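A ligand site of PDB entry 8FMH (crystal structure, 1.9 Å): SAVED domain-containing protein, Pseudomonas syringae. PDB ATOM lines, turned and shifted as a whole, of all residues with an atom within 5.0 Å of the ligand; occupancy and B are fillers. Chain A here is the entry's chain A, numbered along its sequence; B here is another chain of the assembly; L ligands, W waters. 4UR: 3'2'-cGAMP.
The side-chain hydroxyl (OG) of Ser 277 is in hydrogen-bond range of an oxygen (O16) of the ligand.
An oxygen (O44) of the ligand sits at hydrogen-bond distance from the guanidinium group of Arg 366.
An oxygen (O25) of the ligand sits at hydrogen-bond distance from a ring nitrogen (NE2) of His 138.
N of His 357 of chain B lies within hydrogen-bond range of O30 of the ligand, 2.8 Å away.
NH1 of Arg 242 is in salt-bridge range of O15 of the ligand, 3.0 Å away.
A nitrogen (N01) of the ligand is in hydrogen-bond range of the side-chain hydroxyl (OH) of Tyr 304.
The side-chain carboxylate (OD1) of Asp 231 of chain B is in hydrogen-bond range of a nitrogen (N38) of the ligand (2.9 Å).
N35 of the ligand sits at hydrogen-bond distance from NH2 of Arg 232 of chain B (2.8 Å).
O of Ile 341 sits at hydrogen-bond distance from O20 of the ligand (2.9 Å).
The backbone NH of Ala 343 sits at hydrogen-bond distance from an oxygen (O20) of the ligand, 3.0 Å away.
N of Gln 356 of chain B sits at hydrogen-bond distance from O26 of the ligand, at 2.6 Å.
O of Asp 231 of chain B is in hydrogen-bond range of N38 of the ligand.
NH2 of Arg 232 of chain B is in salt-bridge range of OD1 of Asp 231 of chain B (3.2 Å).
NE2 of Gln 321 of chain B is in hydrogen-bond range of O of Ser 277 (3.0 Å).
The guanidinium group (NE) of Arg 242 lies within salt-bridge range of the side-chain carboxylate (OD2) of Asp 231 of chain B (2.8 Å).
NE2 of Gln 356 of chain B sits at hydrogen-bond distance from O of Arg 366 (2.8 Å).
A ring nitrogen (NE2) of His 357 of chain B is in hydrogen-bond range of the side-chain carboxylate of Glu 328 of chain B (2.7 Å).
The side-chain hydroxyl (OG1) of Thr 355 of chain B is in hydrogen-bond range of the backbone carbonyl oxygen (O) of His 357 of chain B, at 3.0 Å.
O of Ile 341 sits close to OG of Ser 277 (3.4 Å).
NH2 of Arg 178 is in hydrogen-bond range of O of Arg 366, at 3.2 Å.
Merely in contact with the ligand: Ala 217 (3.1 Å), Thr 355 of chain B (3.1 Å), Pro 342 (3.2 Å), Ala 278 (3.4 Å), Phe 139 (3.4 Å), Ile 219 (3.5 Å), Phe 374 (3.5 Å), Phe 240 (3.5 Å), Ala 340 (3.6 Å), Pro 281 (3.7 Å), Leu 216 (3.7 Å), Ala 339 (3.7 Å), Gln 279 (3.7 Å) and Val 280 (3.97 Å).
Hydrophobic or aromatic side chains within 4 Å of the ligand: His 138, Phe 139, Leu 216, Ile 219, Phe 240, Ala 278, Pro 281, Tyr 304, Ala 340, Ala 343, Phe 374 and His 357 of chain B.
25 residues have an atom within 4 Å of the ligand: His 138, Phe 139, Leu 216, Ala 217, Ile 219, Phe 240, Arg 242, Ser 277, Ala 278, Gln 279, Val 280, Pro 281, Tyr 304, Ala 339, Ala 340, Ile 341, Pro 342, Ala 343, Arg 366, Phe 374, Asp 231 of chain B, Arg 232 of chain B, Thr 355 of chain B, Gln 356 of chain B and His 357 of chain B.
Water W5 bridges OD1 of Asp 365 (2.5 Å) and O30 of the ligand (2.7 Å).
Water W3 lies within hydrogen-bond range of a nitrogen (N41) of the ligand (2.7 Å) and the backbone NH (N) of Ala 343 (3.0 Å).
Water W2 lies within hydrogen-bond range of the backbone carbonyl oxygen of Tyr 304 (2.6 Å) and an oxygen (O16) of the ligand (2.8 Å).
Water W4 bridges the side-chain carboxylate (OD1) of Asp 365 (2.6 Å) and the backbone carbonyl oxygen (O) of Ala 339 (3.0 Å).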
ATOM      1  N   HIS A 138      12.632   1.798  -8.283  1.00  0.00           N
ATOM      2  CA  HIS A 138      11.661   1.938  -9.363  1.00  0.00           C
ATOM      3  C   HIS A 138      12.246   2.545 -10.620  1.00  0.00           C
ATOM      4  O   HIS A 138      11.554   2.587 -11.649  1.00  0.00           O
ATOM      5  CB  HIS A 138      10.457   2.768  -8.888  1.00  0.00           C
ATOM      6  CG  HIS A 138      10.686   4.244  -8.898  1.00  0.00           C
ATOM      7  ND1 HIS A 138      11.475   4.884  -7.967  1.00  0.00           N
ATOM      8  CD2 HIS A 138      10.191   5.215  -9.703  1.00  0.00           C
ATOM      9  CE1 HIS A 138      11.482   6.181  -8.214  1.00  0.00           C
ATOM     10  NE2 HIS A 138      10.706   6.409  -9.265  1.00  0.00           N
ATOM     11  N   PHE A 139      13.498   2.997 -10.588  1.00  0.00           N
ATOM     12  CA  PHE A 139      14.182   3.403 -11.802  1.00  0.00           C
ATOM     13  C   PHE A 139      14.692   2.176 -12.561  1.00  0.00           C
ATOM     14  O   PHE A 139      14.902   1.109 -11.987  1.00  0.00           O
ATOM     15  CB  PHE A 139      15.355   4.327 -11.480  1.00  0.00           C
ATOM     16  CG  PHE A 139      14.970   5.506 -10.638  1.00  0.00           C
ATOM     17  CD1 PHE A 139      14.461   6.643 -11.225  1.00  0.00           C
ATOM     18  CD2 PHE A 139      15.112   5.467  -9.273  1.00  0.00           C
ATOM     19  CE1 PHE A 139      14.101   7.727 -10.463  1.00  0.00           C
ATOM     20  CE2 PHE A 139      14.769   6.548  -8.496  1.00  0.00           C
ATOM     21  CZ  PHE A 139      14.253   7.688  -9.095  1.00  0.00           C
ATOM     22  N   ARG A 178       4.108  -0.446 -10.547  1.00  0.00           N
ATOM     23  CA  ARG A 178       3.867   0.046  -9.195  1.00  0.00           C
ATOM     24  C   ARG A 178       2.391  -0.146  -8.861  1.00  0.00           C
ATOM     25  O   ARG A 178       1.581   0.785  -8.881  1.00  0.00           O
ATOM     26  CB  ARG A 178       4.302   1.502  -9.062  1.00  0.00           C
ATOM     27  CG  ARG A 178       5.802   1.700  -9.284  1.00  0.00           C
ATOM     28  CD  ARG A 178       6.288   3.057  -8.805  1.00  0.00           C
ATOM     29  NE  ARG A 178       5.696   4.159  -9.547  1.00  0.00           N
ATOM     30  CZ  ARG A 178       6.003   5.435  -9.362  1.00  0.00           C
ATOM     31  NH1 ARG A 178       6.910   5.804  -8.482  1.00  0.00           N
ATOM     32  NH2 ARG A 178       5.367   6.364 -10.080  1.00  0.00           N
ATOM     33  N   LEU A 216      16.129   9.375  -2.147  1.00  0.00           N
ATOM     34  CA  LEU A 216      16.055   9.344  -3.602  1.00  0.00           C
ATOM     35  C   LEU A 216      15.137   8.168  -3.949  1.00  0.00           C
ATOM     36  O   LEU A 216      15.610   7.043  -4.162  1.00  0.00           O
ATOM     37  CB  LEU A 216      17.430   9.226  -4.242  1.00  0.00           C
ATOM     38  CG  LEU A 216      17.547   9.818  -5.646  1.00  0.00           C
ATOM     39  CD1 LEU A 216      18.993   9.830  -6.127  1.00  0.00           C
ATOM     40  CD2 LEU A 216      16.668   9.068  -6.630  1.00  0.00           C
ATOM     41  N   ALA A 217      13.839   8.440  -4.012  1.00  0.00           N
ATOM     42  CA  ALA A 217      12.826   7.404  -4.120  1.00  0.00           C
ATOM     43  C   ALA A 217      11.576   8.011  -4.723  1.00  0.00           C
ATOM     44  O   ALA A 217      11.525   9.206  -5.022  1.00  0.00           O
ATOM     45  CB  ALA A 217      12.530   6.793  -2.744  1.00  0.00           C
ATOM     46  N   ASP A 218      10.544   7.180  -4.893  1.00  0.00           N
ATOM     47  CA  ASP A 218       9.279   7.622  -5.472  1.00  0.00           C
ATOM     48  C   ASP A 218       8.828   8.908  -4.806  1.00  0.00           C
ATOM     49  O   ASP A 218       8.822   9.018  -3.577  1.00  0.00           O
ATOM     50  CB  ASP A 218       8.204   6.552  -5.296  1.00  0.00           C
ATOM     51  CG  ASP A 218       8.656   5.174  -5.719  1.00  0.00           C
ATOM     52  OD1 ASP A 218       9.539   4.599  -5.041  1.00  0.00           O
ATOM     53  OD2 ASP A 218       8.119   4.644  -6.707  1.00  0.00           O
ATOM     54  N   ILE A 219       8.419   9.889  -5.614  1.00  0.00           N
ATOM     55  CA  ILE A 219       7.922  11.140  -5.057  1.00  0.00           C
ATOM     56  C   ILE A 219       6.828  10.909  -4.024  1.00  0.00           C
ATOM     57  O   ILE A 219       6.863  11.539  -2.959  1.00  0.00           O
ATOM     58  CB  ILE A 219       7.481  12.087  -6.197  1.00  0.00           C
ATOM     59  CG1 ILE A 219       8.713  12.738  -6.843  1.00  0.00           C
ATOM     60  CG2 ILE A 219       6.539  13.156  -5.650  1.00  0.00           C
ATOM     61  CD1 ILE A 219       8.406  13.525  -8.116  1.00  0.00           C
ATOM     62  N   LEU A 222       8.530   9.551  -0.781  1.00  0.00           N
ATOM     63  CA  LEU A 222       9.272  10.565  -0.026  1.00  0.00           C
ATOM     64  C   LEU A 222       8.321  11.509   0.701  1.00  0.00           C
ATOM     65  O   LEU A 222       8.619  11.946   1.825  1.00  0.00           O
ATOM     66  CB  LEU A 222      10.180  11.345  -0.973  1.00  0.00           C
ATOM     67  CG  LEU A 222      11.338  10.551  -1.571  1.00  0.00           C
ATOM     68  CD1 LEU A 222      12.043  11.415  -2.597  1.00  0.00           C
ATOM     69  CD2 LEU A 222      12.310  10.099  -0.504  1.00  0.00           C
ATOM     70  N   PHE A 240      20.791  14.561  -2.634  1.00  0.00           N
ATOM     71  CA  PHE A 240      21.659  13.983  -3.654  1.00  0.00           C
ATOM     72  C   PHE A 240      21.555  14.833  -4.917  1.00  0.00           C
ATOM     73  O   PHE A 240      20.456  15.138  -5.384  1.00  0.00           O
ATOM     74  CB  PHE A 240      21.278  12.536  -3.949  1.00  0.00           C
ATOM     75  CG  PHE A 240      22.163  11.860  -4.962  1.00  0.00           C
ATOM     76  CD1 PHE A 240      21.952  12.035  -6.321  1.00  0.00           C
ATOM     77  CD2 PHE A 240      23.197  11.033  -4.567  1.00  0.00           C
ATOM     78  CE1 PHE A 240      22.763  11.411  -7.253  1.00  0.00           C
ATOM     79  CE2 PHE A 240      24.007  10.396  -5.494  1.00  0.00           C
ATOM     80  CZ  PHE A 240      23.790  10.598  -6.843  1.00  0.00           C
ATOM     81  N   ARG A 242      22.980  15.497  -8.963  1.00  0.00           N
ATOM     82  CA  ARG A 242      23.577  14.789 -10.088  1.00  0.00           C
ATOM     83  C   ARG A 242      25.031  15.191 -10.324  1.00  0.00           C
ATOM     84  O   ARG A 242      25.810  14.389 -10.835  1.00  0.00           O
ATOM     85  CB  ARG A 242      22.770  15.041 -11.365  1.00  0.00           C
ATOM     86  CG  ARG A 242      21.479  14.272 -11.447  1.00  0.00           C
ATOM     87  CD  ARG A 242      20.676  14.756 -12.642  1.00  0.00           C
ATOM     88  NE  ARG A 242      19.464  13.968 -12.858  1.00  0.00           N
ATOM     89  CZ  ARG A 242      18.368  14.058 -12.124  1.00  0.00           C
ATOM     90  NH1 ARG A 242      18.291  14.872 -11.091  1.00  0.00           N
ATOM     91  NH2 ARG A 242      17.316  13.312 -12.444  1.00  0.00           N
ATOM     92  N   SER A 277      11.230  20.941 -10.657  1.00  0.00           N
ATOM     93  CA  SER A 277      12.237  20.259 -11.466  1.00  0.00           C
ATOM     94  C   SER A 277      11.947  20.413 -12.960  1.00  0.00           C
ATOM     95  O   SER A 277      12.863  20.317 -13.784  1.00  0.00           O
ATOM     96  CB  SER A 277      12.277  18.770 -11.119  1.00  0.00           C
ATOM     97  OG  SER A 277      12.632  18.554  -9.769  1.00  0.00           O
ATOM     98  N   ALA A 278      10.692  20.644 -13.324  1.00  0.00           N
ATOM     99  CA  ALA A 278      10.298  20.746 -14.714  1.00  0.00           C
ATOM    100  C   ALA A 278       8.901  21.350 -14.761  1.00  0.00           C
ATOM    101  O   ALA A 278       8.229  21.487 -13.731  1.00  0.00           O
ATOM    102  CB  ALA A 278      10.341  19.392 -15.408  1.00  0.00           C
ATOM    103  N   GLN A 279       8.480  21.736 -15.964  1.00  0.00           N
ATOM    104  CA  GLN A 279       7.141  22.268 -16.162  1.00  0.00           C
ATOM    105  C   GLN A 279       6.185  21.098 -16.403  1.00  0.00           C
ATOM    106  O   GLN A 279       6.329  20.362 -17.370  1.00  0.00           O
ATOM    107  CB  GLN A 279       7.105  23.233 -17.342  1.00  0.00           C
ATOM    108  CG  GLN A 279       5.735  23.857 -17.599  1.00  0.00           C
ATOM    109  CD  GLN A 279       5.278  24.771 -16.476  1.00  0.00           C
ATOM    110  OE1 GLN A 279       5.922  25.785 -16.182  1.00  0.00           O
ATOM    111  NE2 GLN A 279       4.163  24.428 -15.851  1.00  0.00           N
ATOM    112  N   VAL A 280       5.232  20.933 -15.490  1.00  0.00           N
ATOM    113  CA  VAL A 280       4.192  19.921 -15.619  1.00  0.00           C
ATOM    114  C   VAL A 280       3.186  20.409 -16.656  1.00  0.00           C
ATOM    115  O   VAL A 280       2.526  21.433 -16.430  1.00  0.00           O
ATOM    116  CB  VAL A 280       3.511  19.648 -14.264  1.00  0.00           C
ATOM    117  CG1 VAL A 280       2.467  18.546 -14.388  1.00  0.00           C
ATOM    118  CG2 VAL A 280       4.557  19.263 -13.214  1.00  0.00           C
ATOM    119  N   PRO A 281       3.031  19.725 -17.792  1.00  0.00           N
ATOM    120  CA  PRO A 281       2.044  20.177 -18.782  1.00  0.00           C
ATOM    121  C   PRO A 281       0.624  20.138 -18.215  1.00  0.00           C
ATOM    122  O   PRO A 281       0.224  19.153 -17.583  1.00  0.00           O
ATOM    123  CB  PRO A 281       2.220  19.189 -19.932  1.00  0.00           C
ATOM    124  CG  PRO A 281       3.605  18.674 -19.781  1.00  0.00           C
ATOM    125  CD  PRO A 281       3.840  18.614 -18.306  1.00  0.00           C
ATOM    126  N   TYR A 304      16.432  20.464 -12.660  1.00  0.00           N
ATOM    127  CA  TYR A 304      16.816  19.337 -11.799  1.00  0.00           C
ATOM    128  C   TYR A 304      17.844  19.736 -10.756  1.00  0.00           C
ATOM    129  O   TYR A 304      17.924  19.101  -9.698  1.00  0.00           O
ATOM    130  CB  TYR A 304      17.380  18.200 -12.648  1.00  0.00           C
ATOM    131  CG  TYR A 304      16.369  17.358 -13.407  1.00  0.00           C
ATOM    132  CD1 TYR A 304      15.032  17.732 -13.505  1.00  0.00           C
ATOM    133  CD2 TYR A 304      16.761  16.181 -14.020  1.00  0.00           C
ATOM    134  CE1 TYR A 304      14.132  16.955 -14.201  1.00  0.00           C
ATOM    135  CE2 TYR A 304      15.858  15.400 -14.707  1.00  0.00           C
ATOM    136  CZ  TYR A 304      14.547  15.786 -14.792  1.00  0.00           C
ATOM    137  OH  TYR A 304      13.658  14.988 -15.483  1.00  0.00           O
ATOM    138  N   ALA A 339       3.317  16.699  -8.917  1.00  0.00           N
ATOM    139  CA  ALA A 339       4.569  17.331  -8.498  1.00  0.00           C
ATOM    140  C   ALA A 339       5.718  16.859  -9.375  1.00  0.00           C
ATOM    141  O   ALA A 339       5.972  15.657  -9.484  1.00  0.00           O
ATOM    142  CB  ALA A 339       4.871  17.027  -7.033  1.00  0.00           C
ATOM    143  N   ALA A 340       6.426  17.822  -9.970  1.00  0.00           N
ATOM    144  CA  ALA A 340       7.727  17.602 -10.587  1.00  0.00           C
ATOM    145  C   ALA A 340       8.734  18.376  -9.735  1.00  0.00           C
ATOM    146  O   ALA A 340       9.052  19.537 -10.018  1.00  0.00           O
ATOM    147  CB  ALA A 340       7.747  18.049 -12.039  1.00  0.00           C
ATOM    148  N   ILE A 341       9.202  17.734  -8.666  1.00  0.00           N
ATOM    149  CA  ILE A 341      10.033  18.405  -7.674  1.00  0.00           C
ATOM    150  C   ILE A 341      11.233  17.508  -7.374  1.00  0.00           C
ATOM    151  O   ILE A 341      11.182  16.298  -7.612  1.00  0.00           O
ATOM    152  CB  ILE A 341       9.235  18.709  -6.381  1.00  0.00           C
ATOM    153  CG1 ILE A 341       8.797  17.406  -5.709  1.00  0.00           C
ATOM    154  CG2 ILE A 341       8.004  19.541  -6.731  1.00  0.00           C
ATOM    155  CD1 ILE A 341       7.996  17.621  -4.445  1.00  0.00           C
ATOM    156  N   PRO A 342      12.328  18.091  -6.888  1.00  0.00           N
ATOM    157  CA  PRO A 342      13.465  17.260  -6.452  1.00  0.00           C
ATOM    158  C   PRO A 342      13.127  16.451  -5.212  1.00  0.00           C
ATOM    159  O   PRO A 342      12.181  16.749  -4.477  1.00  0.00           O
ATOM    160  CB  PRO A 342      14.570  18.285  -6.175  1.00  0.00           C
ATOM    161  CG  PRO A 342      14.177  19.491  -6.934  1.00  0.00           C
ATOM    162  CD  PRO A 342      12.687  19.518  -6.926  1.00  0.00           C
ATOM    163  N   ALA A 343      13.953  15.437  -4.963  1.00  0.00           N
ATOM    164  CA  ALA A 343      13.644  14.469  -3.921  1.00  0.00           C
ATOM    165  C   ALA A 343      13.644  15.101  -2.537  1.00  0.00           C
ATOM    166  O   ALA A 343      12.908  14.646  -1.655  1.00  0.00           O
ATOM    167  CB  ALA A 343      14.647  13.311  -3.967  1.00  0.00           C
ATOM    168  N   ALA A 346      10.326  16.891  -1.938  1.00  0.00           N
ATOM    169  CA  ALA A 346       9.264  15.921  -1.702  1.00  0.00           C
ATOM    170  C   ALA A 346       9.224  15.481  -0.252  1.00  0.00           C
ATOM    171  O   ALA A 346       8.146  15.275   0.321  1.00  0.00           O
ATOM    172  CB  ALA A 346       9.429  14.729  -2.639  1.00  0.00           C
ATOM    173  N   ASP A 365       1.207  10.453  -9.842  1.00  0.00           N
ATOM    174  CA  ASP A 365       2.592  10.306 -10.286  1.00  0.00           C
ATOM    175  C   ASP A 365       2.605   9.705 -11.687  1.00  0.00           C
ATOM    176  O   ASP A 365       1.629   9.106 -12.145  1.00  0.00           O
ATOM    177  CB  ASP A 365       3.414   9.445  -9.323  1.00  0.00           C
ATOM    178  CG  ASP A 365       4.912   9.616  -9.502  1.00  0.00           C
ATOM    179  OD1 ASP A 365       5.339  10.485 -10.303  1.00  0.00           O
ATOM    180  OD2 ASP A 365       5.673   8.884  -8.828  1.00  0.00           O
ATOM    181  N   ARG A 366       3.742   9.875 -12.360  1.00  0.00           N
ATOM    182  CA  ARG A 366       3.890   9.411 -13.726  1.00  0.00           C
ATOM    183  C   ARG A 366       3.909   7.893 -13.774  1.00  0.00           C
ATOM    184  O   ARG A 366       4.668   7.241 -13.055  1.00  0.00           O
ATOM    185  CB  ARG A 366       5.172   9.972 -14.340  1.00  0.00           C
ATOM    186  CG  ARG A 366       5.151  11.471 -14.529  1.00  0.00           C
ATOM    187  CD  ARG A 366       4.230  11.862 -15.664  1.00  0.00           C
ATOM    188  NE  ARG A 366       4.323  13.269 -16.007  1.00  0.00           N
ATOM    189  CZ  ARG A 366       3.713  13.823 -17.044  1.00  0.00           C
ATOM    190  NH1 ARG A 366       2.957  13.117 -17.870  1.00  0.00           N
ATOM    191  NH2 ARG A 366       3.869  15.132 -17.264  1.00  0.00           N
ATOM    192  N   PHE A 374      -0.382  10.600 -15.669  1.00  0.00           N
ATOM    193  CA  PHE A 374      -0.524  10.719 -14.227  1.00  0.00           C
ATOM    194  C   PHE A 374      -1.638   9.792 -13.760  1.00  0.00           C
ATOM    195  O   PHE A 374      -2.741   9.804 -14.291  1.00  0.00           O
ATOM    196  CB  PHE A 374      -0.837  12.158 -13.826  1.00  0.00           C
ATOM    197  CG  PHE A 374       0.380  13.041 -13.714  1.00  0.00           C
ATOM    198  CD1 PHE A 374       1.231  12.929 -12.634  1.00  0.00           C
ATOM    199  CD2 PHE A 374       0.659  13.989 -14.694  1.00  0.00           C
ATOM    200  CE1 PHE A 374       2.353  13.742 -12.537  1.00  0.00           C
ATOM    201  CE2 PHE A 374       1.771  14.801 -14.600  1.00  0.00           C
ATOM    202  CZ  PHE A 374       2.622  14.676 -13.515  1.00  0.00           C
ATOM    203  N   ASP B 231      22.037   8.340 -13.623  1.00  0.00           N
ATOM    204  CA  ASP B 231      22.758   9.437 -12.985  1.00  0.00           C
ATOM    205  C   ASP B 231      22.432   9.531 -11.497  1.00  0.00           C
ATOM    206  O   ASP B 231      22.513  10.615 -10.909  1.00  0.00           O
ATOM    207  CB  ASP B 231      22.447  10.781 -13.682  1.00  0.00           C
ATOM    208  CG  ASP B 231      20.959  11.044 -13.806  1.00  0.00           C
ATOM    209  OD1 ASP B 231      20.151  10.294 -13.225  1.00  0.00           O
ATOM    210  OD2 ASP B 231      20.596  12.024 -14.499  1.00  0.00           O
ATOM    211  N   ARG B 232      22.080   8.409 -10.877  1.00  0.00           N
ATOM    212  CA  ARG B 232      21.697   8.389  -9.468  1.00  0.00           C
ATOM    213  C   ARG B 232      22.552   7.398  -8.689  1.00  0.00           C
ATOM    214  O   ARG B 232      22.034   6.608  -7.891  1.00  0.00           O
ATOM    215  CB  ARG B 232      20.209   8.040  -9.332  1.00  0.00           C
ATOM    216  CG  ARG B 232      19.761   6.818 -10.114  1.00  0.00           C
ATOM    217  CD  ARG B 232      18.253   6.714 -10.204  1.00  0.00           C
ATOM    218  NE  ARG B 232      17.675   7.914 -10.795  1.00  0.00           N
ATOM    219  CZ  ARG B 232      17.592   8.142 -12.104  1.00  0.00           C
ATOM    220  NH1 ARG B 232      17.977   7.230 -12.986  1.00  0.00           N
ATOM    221  NH2 ARG B 232      17.134   9.308 -12.538  1.00  0.00           N
ATOM    222  N   GLN B 321      18.518  19.992 -19.830  1.00  0.00           N
ATOM    223  CA  GLN B 321      17.294  19.639 -19.129  1.00  0.00           C
ATOM    224  C   GLN B 321      16.374  20.850 -19.000  1.00  0.00           C
ATOM    225  O   GLN B 321      15.147  20.712 -19.066  1.00  0.00           O
ATOM    226  CB  GLN B 321      17.609  19.055 -17.751  1.00  0.00           C
ATOM    227  CG  GLN B 321      16.386  18.510 -17.032  1.00  0.00           C
ATOM    228  CD  GLN B 321      15.664  19.550 -16.194  1.00  0.00           C
ATOM    229  OE1 GLN B 321      16.286  20.377 -15.535  1.00  0.00           O
ATOM    230  NE2 GLN B 321      14.335  19.511 -16.235  1.00  0.00           N
ATOM    231  N   GLU B 328       9.284  19.814 -23.803  1.00  0.00           N
ATOM    232  CA  GLU B 328       8.330  18.761 -23.458  1.00  0.00           C
ATOM    233  C   GLU B 328       6.958  19.338 -23.135  1.00  0.00           C
ATOM    234  O   GLU B 328       5.931  18.712 -23.438  1.00  0.00           O
ATOM    235  CB  GLU B 328       8.863  17.939 -22.280  1.00  0.00           C
ATOM    236  CG  GLU B 328       9.966  16.967 -22.701  1.00  0.00           C
ATOM    237  CD  GLU B 328      10.447  16.076 -21.569  1.00  0.00           C
ATOM    238  OE1 GLU B 328       9.845  16.125 -20.468  1.00  0.00           O
ATOM    239  OE2 GLU B 328      11.419  15.315 -21.788  1.00  0.00           O
ATOM    240  N   THR B 355      14.563   9.157 -15.625  1.00  0.00           N
ATOM    241  CA  THR B 355      13.591   9.301 -14.557  1.00  0.00           C
ATOM    242  C   THR B 355      12.359   8.438 -14.846  1.00  0.00           C
ATOM    243  O   THR B 355      12.235   7.830 -15.905  1.00  0.00           O
ATOM    244  CB  THR B 355      13.173  10.770 -14.412  1.00  0.00           C
ATOM    245  OG1 THR B 355      12.785  11.287 -15.683  1.00  0.00           O
ATOM    246  CG2 THR B 355      14.313  11.592 -13.840  1.00  0.00           C
ATOM    247  N   GLN B 356      11.455   8.399 -13.863  1.00  0.00           N
ATOM    248  CA  GLN B 356      10.160   7.762 -14.093  1.00  0.00           C
ATOM    249  C   GLN B 356       9.434   8.437 -15.258  1.00  0.00           C
ATOM    250  O   GLN B 356       8.911   7.754 -16.152  1.00  0.00           O
ATOM    251  CB  GLN B 356       9.331   7.830 -12.801  1.00  0.00           C
ATOM    252  CG  GLN B 356       7.910   7.303 -12.906  1.00  0.00           C
ATOM    253  CD  GLN B 356       7.829   5.807 -13.042  1.00  0.00           C
ATOM    254  OE1 GLN B 356       8.836   5.098 -12.944  1.00  0.00           O
ATOM    255  NE2 GLN B 356       6.635   5.310 -13.293  1.00  0.00           N
ATOM    256  N   HIS B 357       9.409   9.766 -15.263  1.00  0.00           N
ATOM    257  CA  HIS B 357       8.836  10.495 -16.392  1.00  0.00           C
ATOM    258  C   HIS B 357       9.617  10.191 -17.668  1.00  0.00           C
ATOM    259  O   HIS B 357      10.849  10.145 -17.660  1.00  0.00           O
ATOM    260  CB  HIS B 357       8.863  11.997 -16.133  1.00  0.00           C
ATOM    261  CG  HIS B 357       8.624  12.815 -17.361  1.00  0.00           C
ATOM    262  ND1 HIS B 357       7.386  12.920 -17.958  1.00  0.00           N
ATOM    263  CD2 HIS B 357       9.467  13.571 -18.111  1.00  0.00           C
ATOM    264  CE1 HIS B 357       7.472  13.702 -19.014  1.00  0.00           C
ATOM    265  NE2 HIS B 357       8.727  14.113 -19.135  1.00  0.00           N
HETATM  266  C21 4UR L   1      12.393  11.415  -7.137  1.00  0.00           C
HETATM  267  C22 4UR L   1      11.828  10.260  -7.935  1.00  0.00           C
HETATM  268  C28 4UR L   1      10.894  12.606 -11.460  1.00  0.00           C
HETATM  269  N01 4UR L   1      10.923  16.138 -16.108  1.00  0.00           N
HETATM  270  C02 4UR L   1       9.725  15.863 -15.568  1.00  0.00           C
HETATM  271  N03 4UR L   1       9.647  15.141 -14.460  1.00  0.00           N
HETATM  272  C04 4UR L   1       8.358  14.962 -14.052  1.00  0.00           C
HETATM  273  C05 4UR L   1       7.210  15.433 -14.640  1.00  0.00           C
HETATM  274  N06 4UR L   1       6.096  15.040 -13.912  1.00  0.00           N
HETATM  275  C07 4UR L   1       6.582  14.341 -12.909  1.00  0.00           C
HETATM  276  N08 4UR L   1       7.953  14.258 -12.955  1.00  0.00           N
HETATM  277  C09 4UR L   1       8.822  13.571 -11.991  1.00  0.00           C
HETATM  278  O10 4UR L   1       9.545  14.537 -11.263  1.00  0.00           O
HETATM  279  C11 4UR L   1      10.883  14.048 -10.978  1.00  0.00           C
HETATM  280  C12 4UR L   1      11.875  14.960 -11.647  1.00  0.00           C
HETATM  281  O13 4UR L   1      13.225  14.466 -11.429  1.00  0.00           O
HETATM  282  P14 4UR L   1      14.116  14.971 -10.198  1.00  0.00           P
HETATM  283  O15 4UR L   1      15.458  14.308 -10.285  1.00  0.00           O
HETATM  284  O16 4UR L   1      14.102  16.473 -10.190  1.00  0.00           O
HETATM  285  O17 4UR L   1      13.323  14.472  -8.887  1.00  0.00           O
HETATM  286  C18 4UR L   1      13.217  13.061  -8.630  1.00  0.00           C
HETATM  287  C19 4UR L   1      12.071  12.821  -7.661  1.00  0.00           C
HETATM  288  O20 4UR L   1      12.114  13.728  -6.573  1.00  0.00           O
HETATM  289  O23 4UR L   1      12.196  10.379  -9.327  1.00  0.00           O
HETATM  290  P24 4UR L   1      11.048  10.263 -10.439  1.00  0.00           P
HETATM  291  O25 4UR L   1       9.999   9.314  -9.905  1.00  0.00           O
HETATM  292  O26 4UR L   1      11.684   9.978 -11.761  1.00  0.00           O
HETATM  293  O27 4UR L   1      10.427  11.745 -10.417  1.00  0.00           O
HETATM  294  C29 4UR L   1       9.880  12.652 -12.606  1.00  0.00           C
HETATM  295  O30 4UR L   1       9.322  11.409 -12.965  1.00  0.00           O
HETATM  296  O31 4UR L   1      13.838  11.339  -7.157  1.00  0.00           O
HETATM  297  C32 4UR L   1      14.373  12.463  -7.846  1.00  0.00           C
HETATM  298  N33 4UR L   1      15.480  11.980  -8.661  1.00  0.00           N
HETATM  299  C34 4UR L   1      15.416  11.068  -9.689  1.00  0.00           C
HETATM  300  N35 4UR L   1      16.582  10.826 -10.242  1.00  0.00           N
HETATM  301  C36 4UR L   1      17.472  11.600  -9.516  1.00  0.00           C
HETATM  302  C37 4UR L   1      18.856  11.780  -9.612  1.00  0.00           C
HETATM  303  N38 4UR L   1      19.633  11.157 -10.509  1.00  0.00           N
HETATM  304  N39 4UR L   1      19.445  12.627  -8.738  1.00  0.00           N
HETATM  305  C40 4UR L   1      18.668  13.250  -7.842  1.00  0.00           C
HETATM  306  N41 4UR L   1      17.353  13.176  -7.667  1.00  0.00           N
HETATM  307  C42 4UR L   1      16.809  12.318  -8.543  1.00  0.00           C
HETATM  308  C43 4UR L   1       7.299  16.222 -15.828  1.00  0.00           C
HETATM  309  O44 4UR L   1       6.385  16.729 -16.489  1.00  0.00           O
HETATM  310  N45 4UR L   1       8.627  16.382 -16.222  1.00  0.00           N
HETATM  311  O   HOH W   1       6.512  17.338 -19.483  1.00  0.00           O
HETATM  312  O   HOH W   2      16.227  17.397  -8.708  1.00  0.00           O
HETATM  313  O   HOH W   3      16.578  15.445  -6.443  1.00  0.00           O
HETATM  314  O   HOH W   4       4.800  12.998 -10.273  1.00  0.00           O
HETATM  315  O   HOH W   5       7.670  10.298 -11.209  1.00  0.00           O
